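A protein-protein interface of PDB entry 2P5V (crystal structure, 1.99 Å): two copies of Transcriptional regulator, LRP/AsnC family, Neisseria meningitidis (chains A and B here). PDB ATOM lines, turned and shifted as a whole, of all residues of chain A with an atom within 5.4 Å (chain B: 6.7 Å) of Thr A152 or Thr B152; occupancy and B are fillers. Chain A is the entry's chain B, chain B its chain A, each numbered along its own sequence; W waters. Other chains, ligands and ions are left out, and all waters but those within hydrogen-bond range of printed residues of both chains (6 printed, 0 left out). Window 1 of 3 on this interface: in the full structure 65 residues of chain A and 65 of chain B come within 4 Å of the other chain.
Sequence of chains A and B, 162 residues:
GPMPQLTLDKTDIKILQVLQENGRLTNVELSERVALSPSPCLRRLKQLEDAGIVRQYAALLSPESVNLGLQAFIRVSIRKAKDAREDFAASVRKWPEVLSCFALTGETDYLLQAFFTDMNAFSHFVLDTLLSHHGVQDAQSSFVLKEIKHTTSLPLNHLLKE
The backbone carbonyl oxygen of Leu A60 lies within hydrogen-bond range of the backbone NH of Arg B55, 2.9 Å away.
The side-chain amide nitrogen of Gln B56 is in hydrogen-bond range of the backbone carbonyl oxygen of Gln A20, at 3.1 Å.
The backbone carbonyl oxygen (O) of Gln B56 sits at hydrogen-bond distance from the backbone NH (N) of Leu A60 (2.7 Å).
The backbone NH (N) of Ala B58 sits at hydrogen-bond distance from the backbone carbonyl oxygen (O) of Ala A58 (2.9 Å).
The backbone carbonyl oxygen (O) of Leu B99 is in hydrogen-bond range of the backbone NH (N) of Thr A151, at 2.8 Å.
ND1 of His A150 is in hydrogen-bond range of OG of Ser B100 (2.9 Å).
The backbone carbonyl oxygen of Leu A99 is in hydrogen-bond range of the backbone NH of Thr B151.
N of Leu B154 lies within hydrogen-bond range of OE1 of Gln B20, 2.8 Å away.
OG of Ser B153 is in hydrogen-bond range of OE2 of Glu B21.
The side-chain hydroxyl (OG1) of Thr B151 is in hydrogen-bond range of the backbone NH (N) of Ser B153 (3.1 Å).
N of Leu A154 lies within hydrogen-bond range of OE1 of Gln A20 (2.8 Å).
The backbone NH of Ser A153 sits at hydrogen-bond distance from the side-chain hydroxyl of Thr A151 (3.2 Å).
CG of Gln A20 touches O of Ala B59, at 3.5 Å.
CG of Leu B61 touches OE1 of Gln A20, at 3.4 Å.
OG1 of Thr B152 touches CB of Ala A58, at 3.6 Å.
Gln B20 touches Ala A59 (CA to O, 3.5 Å).
O of Gln B56 touches C of Ala A59, 3.6 Å away.
Leu A99 touches Ser B153 (CG to O, 3.2 Å).
NH2 of Arg B55 touches CD2 of His A150, at 3.5 Å.
CA of His A150 touches O of Leu B99, at 3.4 Å.
OG1 of Thr A152 touches CD2 of Leu B60, 3.6 Å away.
O of Ser A153 touches CD1 of Leu B99 (3.2 Å).
Of the printed residues of chain B, Ala A58 touches Gln B20 (3.3 Å), Gln B56 (3.9 Å), Ala B58 (2.9 Å) and Thr B152 (3.6 Å).
Printed residues of chain B within 4 Å of Thr A151: Leu B99.
Of the printed residues of chain B, Thr A152 touches Ala B58, Leu B60 and Thr B152.
Glu B21 touches none of the printed residues of chain A.
Printed residues of chain A within 4 Å of Ala B58: Gln A20 (3.2 Å), Ala A58 (2.9 Å) and Thr A152 (3.7 Å).
Of chain A, only Ala A58 (3.6 Å), Leu A60 (3.4 Å), Leu A99 (3.7 Å) and Thr A152 (3.97 Å) come within 4 Å of Thr B152.
The nearest residue of chain B that does not touch Thr A152 is Leu B99 (4.02 Å).
The nearest printed residue of chain A that does not touch Gln B20 is Leu A60 (5.4 Å).
Of the 10 printed residues of chain A, 10 touch a printed residue of chain B.
Printed residues of chain A that touch a printed residue of chain B: Gln A20, Ala A58, Ala A59, Leu A60, Leu A99, His A150, Thr A151, Thr A152, Ser A153 and Leu A154.
Hydrophobic or aromatic side chains of chain B within 4 Å of the printed part of chain A: Ala B58, Ala B59, Leu B60, Leu B61, Leu B99 and Leu B154.
Among the printed residues, 28 pairs touch across the chains.
Among the printed residues, no Asp or Glu carboxylate lies within 4 Å of a Lys or Arg side-chain nitrogen of the other chain.
Gln A20 touches Ala B58, and with the chains exchanged Ala A58 touches Gln B20.
Leu A99 touches Thr B151, and with the chains exchanged Thr A151 touches Leu B99.
Leu A99 touches Thr B152, but with the chains exchanged Thr A152 does not touch Leu B99 (4.02 Å).
Leu A99 touches Ser B153, and with the chains exchanged Ser A153 touches Leu B99.
10 positions are printed for both chains.
Water W6 lies within hydrogen-bond range of the backbone carbonyl oxygen of Ala B59, the side-chain hydroxyl of Thr A152 and the backbone carbonyl oxygen of Gln A20.
Water W4 lies within hydrogen-bond range of the side-chain hydroxyl (OG1) of Thr B152, the backbone carbonyl oxygen (O) of Gln B20, the backbone carbonyl oxygen (O) of Ala A59 and the side-chain hydroxyl (OG) of Ser B153.
Water W5 lies within hydrogen-bond range of O of Thr A152, OE1 of Gln A20 and N of Leu B61.
Water W2 bridges the side-chain amide oxygen (OE1) of Gln B56 (2.8 Å) and the side-chain hydroxyl (OG1) of Thr A152 (3.1 Å).
Water W1 lies within hydrogen-bond range of NE2 of Gln B56 (2.9 Å), OG1 of Thr A151 (3.0 Å), OG of Ser A153 (3.1 Å), OG1 of Thr A152 (3.3 Å) and O of Gln A20 (3.4 Å).
Water W3 lies within hydrogen-bond range of O of His A150, OE1 of Gln B56 and NH1 of Arg B55.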
ATOM      1  N   GLN A  20     -10.571  19.420  28.053  1.00  0.00           N
ATOM      2  CA  GLN A  20      -9.131  19.244  28.248  1.00  0.00           C
ATOM      3  C   GLN A  20      -8.758  19.025  29.711  1.00  0.00           C
ATOM      4  O   GLN A  20      -7.840  18.256  30.012  1.00  0.00           O
ATOM      5  CB  GLN A  20      -8.344  20.405  27.679  1.00  0.00           C
ATOM      6  CG  GLN A  20      -8.126  20.300  26.185  1.00  0.00           C
ATOM      7  CD  GLN A  20      -7.125  21.308  25.669  1.00  0.00           C
ATOM      8  OE1 GLN A  20      -6.147  20.939  25.031  1.00  0.00           O
ATOM      9  NE2 GLN A  20      -7.345  22.591  25.976  1.00  0.00           N
ATOM     10  N   ALA A  58      -8.143  10.400  27.692  1.00  0.00           N
ATOM     11  CA  ALA A  58      -7.186   9.616  28.487  1.00  0.00           C
ATOM     12  C   ALA A  58      -7.271   9.949  29.984  1.00  0.00           C
ATOM     13  O   ALA A  58      -7.349  11.125  30.380  1.00  0.00           O
ATOM     14  CB  ALA A  58      -5.746   9.851  27.981  1.00  0.00           C
ATOM     15  N   ALA A  59      -7.258   8.897  30.802  1.00  0.00           N
ATOM     16  CA  ALA A  59      -6.939   9.013  32.222  1.00  0.00           C
ATOM     17  C   ALA A  59      -5.434   9.301  32.349  1.00  0.00           C
ATOM     18  O   ALA A  59      -4.612   8.634  31.718  1.00  0.00           O
ATOM     19  CB  ALA A  59      -7.305   7.730  32.957  1.00  0.00           C
ATOM     20  N   LEU A  60      -5.082  10.322  33.124  1.00  0.00           N
ATOM     21  CA  LEU A  60      -3.676  10.669  33.359  1.00  0.00           C
ATOM     22  C   LEU A  60      -3.318  10.218  34.763  1.00  0.00           C
ATOM     23  O   LEU A  60      -4.050  10.478  35.717  1.00  0.00           O
ATOM     24  CB  LEU A  60      -3.443  12.176  33.192  1.00  0.00           C
ATOM     25  CG  LEU A  60      -3.860  12.805  31.846  1.00  0.00           C
ATOM     26  CD1 LEU A  60      -3.562  14.315  31.833  1.00  0.00           C
ATOM     27  CD2 LEU A  60      -3.143  12.133  30.680  1.00  0.00           C
ATOM     28  N   LEU A  99       7.329   7.526  26.390  1.00  0.00           N
ATOM     29  CA  LEU A  99       6.014   8.114  26.106  1.00  0.00           C
ATOM     30  C   LEU A  99       6.053   9.036  24.899  1.00  0.00           C
ATOM     31  O   LEU A  99       5.072   9.133  24.147  1.00  0.00           O
ATOM     32  CB  LEU A  99       5.465   8.884  27.321  1.00  0.00           C
ATOM     33  CG  LEU A  99       4.616   8.044  28.290  1.00  0.00           C
ATOM     34  CD1 LEU A  99       5.454   6.957  28.918  1.00  0.00           C
ATOM     35  CD2 LEU A  99       3.983   8.924  29.375  1.00  0.00           C
ATOM     36  N   HIS A 150       3.023  20.617  34.553  1.00  0.00           N
ATOM     37  CA  HIS A 150       2.828  19.607  33.548  1.00  0.00           C
ATOM     38  C   HIS A 150       1.360  19.439  33.247  1.00  0.00           C
ATOM     39  O   HIS A 150       0.617  18.849  34.036  1.00  0.00           O
ATOM     40  CB  HIS A 150       3.408  18.277  33.983  1.00  0.00           C
ATOM     41  CG  HIS A 150       3.119  17.177  33.021  1.00  0.00           C
ATOM     42  ND1 HIS A 150       3.512  17.229  31.702  1.00  0.00           N
ATOM     43  CD2 HIS A 150       2.437  16.018  33.169  1.00  0.00           C
ATOM     44  CE1 HIS A 150       3.097  16.140  31.082  1.00  0.00           C
ATOM     45  NE2 HIS A 150       2.444  15.389  31.950  1.00  0.00           N
ATOM     46  N   THR A 151       0.960  19.948  32.088  1.00  0.00           N
ATOM     47  CA  THR A 151      -0.411  19.836  31.630  1.00  0.00           C
ATOM     48  C   THR A 151      -0.409  19.339  30.187  1.00  0.00           C
ATOM     49  O   THR A 151       0.610  19.421  29.487  1.00  0.00           O
ATOM     50  CB  THR A 151      -1.164  21.192  31.767  1.00  0.00           C
ATOM     51  OG1 THR A 151      -2.535  21.027  31.379  1.00  0.00           O
ATOM     52  CG2 THR A 151      -0.533  22.254  30.916  1.00  0.00           C
ATOM     53  N   THR A 152      -1.546  18.783  29.779  1.00  0.00           N
ATOM     54  CA  THR A 152      -1.782  18.363  28.401  1.00  0.00           C
ATOM     55  C   THR A 152      -2.693  19.366  27.648  1.00  0.00           C
ATOM     56  O   THR A 152      -2.861  19.269  26.435  1.00  0.00           O
ATOM     57  CB  THR A 152      -2.387  16.942  28.358  1.00  0.00           C
ATOM     58  OG1 THR A 152      -3.571  16.884  29.164  1.00  0.00           O
ATOM     59  CG2 THR A 152      -1.378  15.934  28.883  1.00  0.00           C
ATOM     60  N   SER A 153      -3.242  20.341  28.368  1.00  0.00           N
ATOM     61  CA  SER A 153      -4.101  21.364  27.776  1.00  0.00           C
ATOM     62  C   SER A 153      -3.336  22.276  26.837  1.00  0.00           C
ATOM     63  O   SER A 153      -2.371  22.919  27.246  1.00  0.00           O
ATOM     64  CB  SER A 153      -4.734  22.239  28.861  1.00  0.00           C
ATOM     65  OG  SER A 153      -5.722  21.534  29.581  1.00  0.00           O
ATOM     66  N   LEU A 154      -3.778  22.331  25.584  1.00  0.00           N
ATOM     67  CA  LEU A 154      -3.234  23.272  24.618  1.00  0.00           C
ATOM     68  C   LEU A 154      -3.887  24.637  24.828  1.00  0.00           C
ATOM     69  O   LEU A 154      -5.068  24.708  25.183  1.00  0.00           O
ATOM     70  CB  LEU A 154      -3.529  22.791  23.205  1.00  0.00           C
ATOM     71  CG  LEU A 154      -2.887  21.474  22.779  1.00  0.00           C
ATOM     72  CD1 LEU A 154      -3.275  21.176  21.355  1.00  0.00           C
ATOM     73  CD2 LEU A 154      -1.379  21.572  22.919  1.00  0.00           C
ATOM     74  N   GLN B  20      -6.334   4.818  30.750  1.00  0.00           N
ATOM     75  CA  GLN B  20      -5.252   5.583  30.122  1.00  0.00           C
ATOM     76  C   GLN B  20      -5.424   5.692  28.605  1.00  0.00           C
ATOM     77  O   GLN B  20      -5.024   6.680  28.001  1.00  0.00           O
ATOM     78  CB  GLN B  20      -3.886   4.964  30.410  1.00  0.00           C
ATOM     79  CG  GLN B  20      -3.304   5.373  31.758  1.00  0.00           C
ATOM     80  CD  GLN B  20      -1.842   5.046  31.844  1.00  0.00           C
ATOM     81  OE1 GLN B  20      -1.026   5.889  32.229  1.00  0.00           O
ATOM     82  NE2 GLN B  20      -1.486   3.821  31.450  1.00  0.00           N
ATOM     83  N   GLU B  21      -5.992   4.659  27.994  1.00  0.00           N
ATOM     84  CA  GLU B  21      -6.239   4.654  26.557  1.00  0.00           C
ATOM     85  C   GLU B  21      -7.614   5.206  26.204  1.00  0.00           C
ATOM     86  O   GLU B  21      -7.784   5.802  25.153  1.00  0.00           O
ATOM     87  CB  GLU B  21      -6.119   3.225  26.009  1.00  0.00           C
ATOM     88  CG  GLU B  21      -4.761   2.568  26.254  1.00  0.00           C
ATOM     89  CD  GLU B  21      -3.578   3.362  25.707  1.00  0.00           C
ATOM     90  OE1 GLU B  21      -3.703   3.981  24.623  1.00  0.00           O
ATOM     91  OE2 GLU B  21      -2.514   3.352  26.368  1.00  0.00           O
ATOM     92  N   ARG B  55      -4.956  11.136  38.387  1.00  0.00           N
ATOM     93  CA  ARG B  55      -4.893  12.532  38.800  1.00  0.00           C
ATOM     94  C   ARG B  55      -5.812  13.410  37.958  1.00  0.00           C
ATOM     95  O   ARG B  55      -6.156  14.505  38.384  1.00  0.00           O
ATOM     96  CB  ARG B  55      -3.459  13.055  38.754  1.00  0.00           C
ATOM     97  CG  ARG B  55      -2.805  13.010  37.399  1.00  0.00           C
ATOM     98  CD  ARG B  55      -1.413  13.608  37.450  1.00  0.00           C
ATOM     99  NE  ARG B  55      -0.756  13.536  36.147  1.00  0.00           N
ATOM    100  CZ  ARG B  55      -1.030  14.324  35.108  1.00  0.00           C
ATOM    101  NH1 ARG B  55      -1.959  15.280  35.182  1.00  0.00           N
ATOM    102  NH2 ARG B  55      -0.366  14.158  33.976  1.00  0.00           N
ATOM    103  N   GLN B  56      -6.196  12.934  36.768  1.00  0.00           N
ATOM    104  CA  GLN B  56      -7.013  13.718  35.831  1.00  0.00           C
ATOM    105  C   GLN B  56      -7.526  12.900  34.644  1.00  0.00           C
ATOM    106  O   GLN B  56      -6.882  11.966  34.203  1.00  0.00           O
ATOM    107  CB  GLN B  56      -6.197  14.895  35.275  1.00  0.00           C
ATOM    108  CG  GLN B  56      -7.040  16.032  34.725  1.00  0.00           C
ATOM    109  CD  GLN B  56      -6.234  16.997  33.884  1.00  0.00           C
ATOM    110  OE1 GLN B  56      -5.084  17.307  34.204  1.00  0.00           O
ATOM    111  NE2 GLN B  56      -6.827  17.471  32.797  1.00  0.00           N
ATOM    112  N   ALA B  58      -8.521  13.805  30.712  1.00  0.00           N
ATOM    113  CA  ALA B  58      -8.307  14.864  29.734  1.00  0.00           C
ATOM    114  C   ALA B  58      -8.726  14.445  28.330  1.00  0.00           C
ATOM    115  O   ALA B  58      -8.362  13.360  27.858  1.00  0.00           O
ATOM    116  CB  ALA B  58      -6.846  15.247  29.709  1.00  0.00           C
ATOM    117  N   ALA B  59      -9.458  15.331  27.664  1.00  0.00           N
ATOM    118  CA  ALA B  59      -9.485  15.368  26.211  1.00  0.00           C
ATOM    119  C   ALA B  59      -8.119  15.847  25.715  1.00  0.00           C
ATOM    120  O   ALA B  59      -7.593  16.869  26.169  1.00  0.00           O
ATOM    121  CB  ALA B  59     -10.567  16.294  25.714  1.00  0.00           C
ATOM    122  N   LEU B  60      -7.539  15.081  24.804  1.00  0.00           N
ATOM    123  CA  LEU B  60      -6.278  15.444  24.180  1.00  0.00           C
ATOM    124  C   LEU B  60      -6.562  15.946  22.774  1.00  0.00           C
ATOM    125  O   LEU B  60      -7.297  15.312  22.014  1.00  0.00           O
ATOM    126  CB  LEU B  60      -5.346  14.241  24.136  1.00  0.00           C
ATOM    127  CG  LEU B  60      -5.087  13.601  25.503  1.00  0.00           C
ATOM    128  CD1 LEU B  60      -4.108  12.437  25.339  1.00  0.00           C
ATOM    129  CD2 LEU B  60      -4.556  14.655  26.502  1.00  0.00           C
ATOM    130  N   LEU B  61      -5.988  17.095  22.432  1.00  0.00           N
ATOM    131  CA  LEU B  61      -6.282  17.722  21.156  1.00  0.00           C
ATOM    132  C   LEU B  61      -5.131  17.598  20.188  1.00  0.00           C
ATOM    133  O   LEU B  61      -3.980  17.412  20.586  1.00  0.00           O
ATOM    134  CB  LEU B  61      -6.659  19.205  21.335  1.00  0.00           C
ATOM    135  CG  LEU B  61      -7.732  19.541  22.385  1.00  0.00           C
ATOM    136  CD1 LEU B  61      -8.204  20.957  22.147  1.00  0.00           C
ATOM    137  CD2 LEU B  61      -8.908  18.561  22.395  1.00  0.00           C
ATOM    138  N   LEU B  99       3.202  24.176  28.386  1.00  0.00           N
ATOM    139  CA  LEU B  99       2.488  23.011  28.902  1.00  0.00           C
ATOM    140  C   LEU B  99       3.237  22.335  30.035  1.00  0.00           C
ATOM    141  O   LEU B  99       2.628  21.895  31.009  1.00  0.00           O
ATOM    142  CB  LEU B  99       2.244  21.983  27.788  1.00  0.00           C
ATOM    143  CG  LEU B  99       0.888  22.107  27.086  1.00  0.00           C
ATOM    144  CD1 LEU B  99       0.720  23.494  26.482  1.00  0.00           C
ATOM    145  CD2 LEU B  99       0.752  20.994  26.029  1.00  0.00           C
ATOM    146  N   SER B 100       4.553  22.230  29.890  1.00  0.00           N
ATOM    147  CA  SER B 100       5.399  21.525  30.851  1.00  0.00           C
ATOM    148  C   SER B 100       6.608  22.369  31.190  1.00  0.00           C
ATOM    149  O   SER B 100       7.131  23.092  30.335  1.00  0.00           O
ATOM    150  CB  SER B 100       5.909  20.185  30.269  1.00  0.00           C
ATOM    151  OG  SER B 100       4.856  19.257  30.077  1.00  0.00           O
ATOM    152  N   HIS B 150       3.934  10.000  20.797  1.00  0.00           N
ATOM    153  CA  HIS B 150       3.461  10.881  21.859  1.00  0.00           C
ATOM    154  C   HIS B 150       2.245  10.253  22.501  1.00  0.00           C
ATOM    155  O   HIS B 150       1.161  10.268  21.930  1.00  0.00           O
ATOM    156  CB  HIS B 150       3.136  12.271  21.315  1.00  0.00           C
ATOM    157  CG  HIS B 150       2.586  13.213  22.341  1.00  0.00           C
ATOM    158  ND1 HIS B 150       3.108  13.322  23.611  1.00  0.00           N
ATOM    159  CD2 HIS B 150       1.575  14.107  22.273  1.00  0.00           C
ATOM    160  CE1 HIS B 150       2.425  14.222  24.290  1.00  0.00           C
ATOM    161  NE2 HIS B 150       1.495  14.723  23.498  1.00  0.00           N
ATOM    162  N   THR B 151       2.437   9.652  23.666  1.00  0.00           N
ATOM    163  CA  THR B 151       1.316   9.105  24.443  1.00  0.00           C
ATOM    164  C   THR B 151       1.421   9.606  25.858  1.00  0.00           C
ATOM    165  O   THR B 151       2.498  10.005  26.287  1.00  0.00           O
ATOM    166  CB  THR B 151       1.222   7.549  24.386  1.00  0.00           C
ATOM    167  OG1 THR B 151       0.160   7.106  25.238  1.00  0.00           O
ATOM    168  CG2 THR B 151       2.494   6.876  24.812  1.00  0.00           C
ATOM    169  N   THR B 152       0.292   9.637  26.561  1.00  0.00           N
ATOM    170  CA  THR B 152       0.261  10.054  27.962  1.00  0.00           C
ATOM    171  C   THR B 152       0.270   8.821  28.877  1.00  0.00           C
ATOM    172  O   THR B 152       0.366   8.934  30.102  1.00  0.00           O
ATOM    173  CB  THR B 152      -0.969  10.970  28.266  1.00  0.00           C
ATOM    174  OG1 THR B 152      -2.191  10.293  27.950  1.00  0.00           O
ATOM    175  CG2 THR B 152      -0.896  12.255  27.464  1.00  0.00           C
ATOM    176  N   SER B 153       0.201   7.643  28.267  1.00  0.00           N
ATOM    177  CA  SER B 153       0.044   6.421  29.007  1.00  0.00           C
ATOM    178  C   SER B 153       1.377   6.031  29.602  1.00  0.00           C
ATOM    179  O   SER B 153       2.367   5.912  28.882  1.00  0.00           O
ATOM    180  CB  SER B 153      -0.477   5.295  28.107  1.00  0.00           C
ATOM    181  OG  SER B 153      -1.688   5.663  27.482  1.00  0.00           O
ATOM    182  N   LEU B 154       1.399   5.852  30.920  1.00  0.00           N
ATOM    183  CA  LEU B 154       2.583   5.377  31.611  1.00  0.00           C
ATOM    184  C   LEU B 154       2.668   3.861  31.458  1.00  0.00           C
ATOM    185  O   LEU B 154       1.641   3.176  31.331  1.00  0.00           O
ATOM    186  CB  LEU B 154       2.544   5.764  33.088  1.00  0.00           C
ATOM    187  CG  LEU B 154       2.468   7.269  33.385  1.00  0.00           C
ATOM    188  CD1 LEU B 154       2.106   7.547  34.852  1.00  0.00           C
ATOM    189  CD2 LEU B 154       3.776   7.933  32.997  1.00  0.00           C
HETATM  190  O   HOH W   1      -4.850  19.067  31.332  1.00  0.00           O
HETATM  191  O   HOH W   2      -3.079  17.475  32.214  1.00  0.00           O
HETATM  192  O   HOH W   3      -2.153  18.667  35.155  1.00  0.00           O
HETATM  193  O   HOH W   4      -2.970   8.057  29.255  1.00  0.00           O
HETATM  194  O   HOH W   5      -4.793  18.528  24.662  1.00  0.00           O
HETATM  195  O   HOH W   6      -5.815  17.779  27.804  1.00  0.00           O
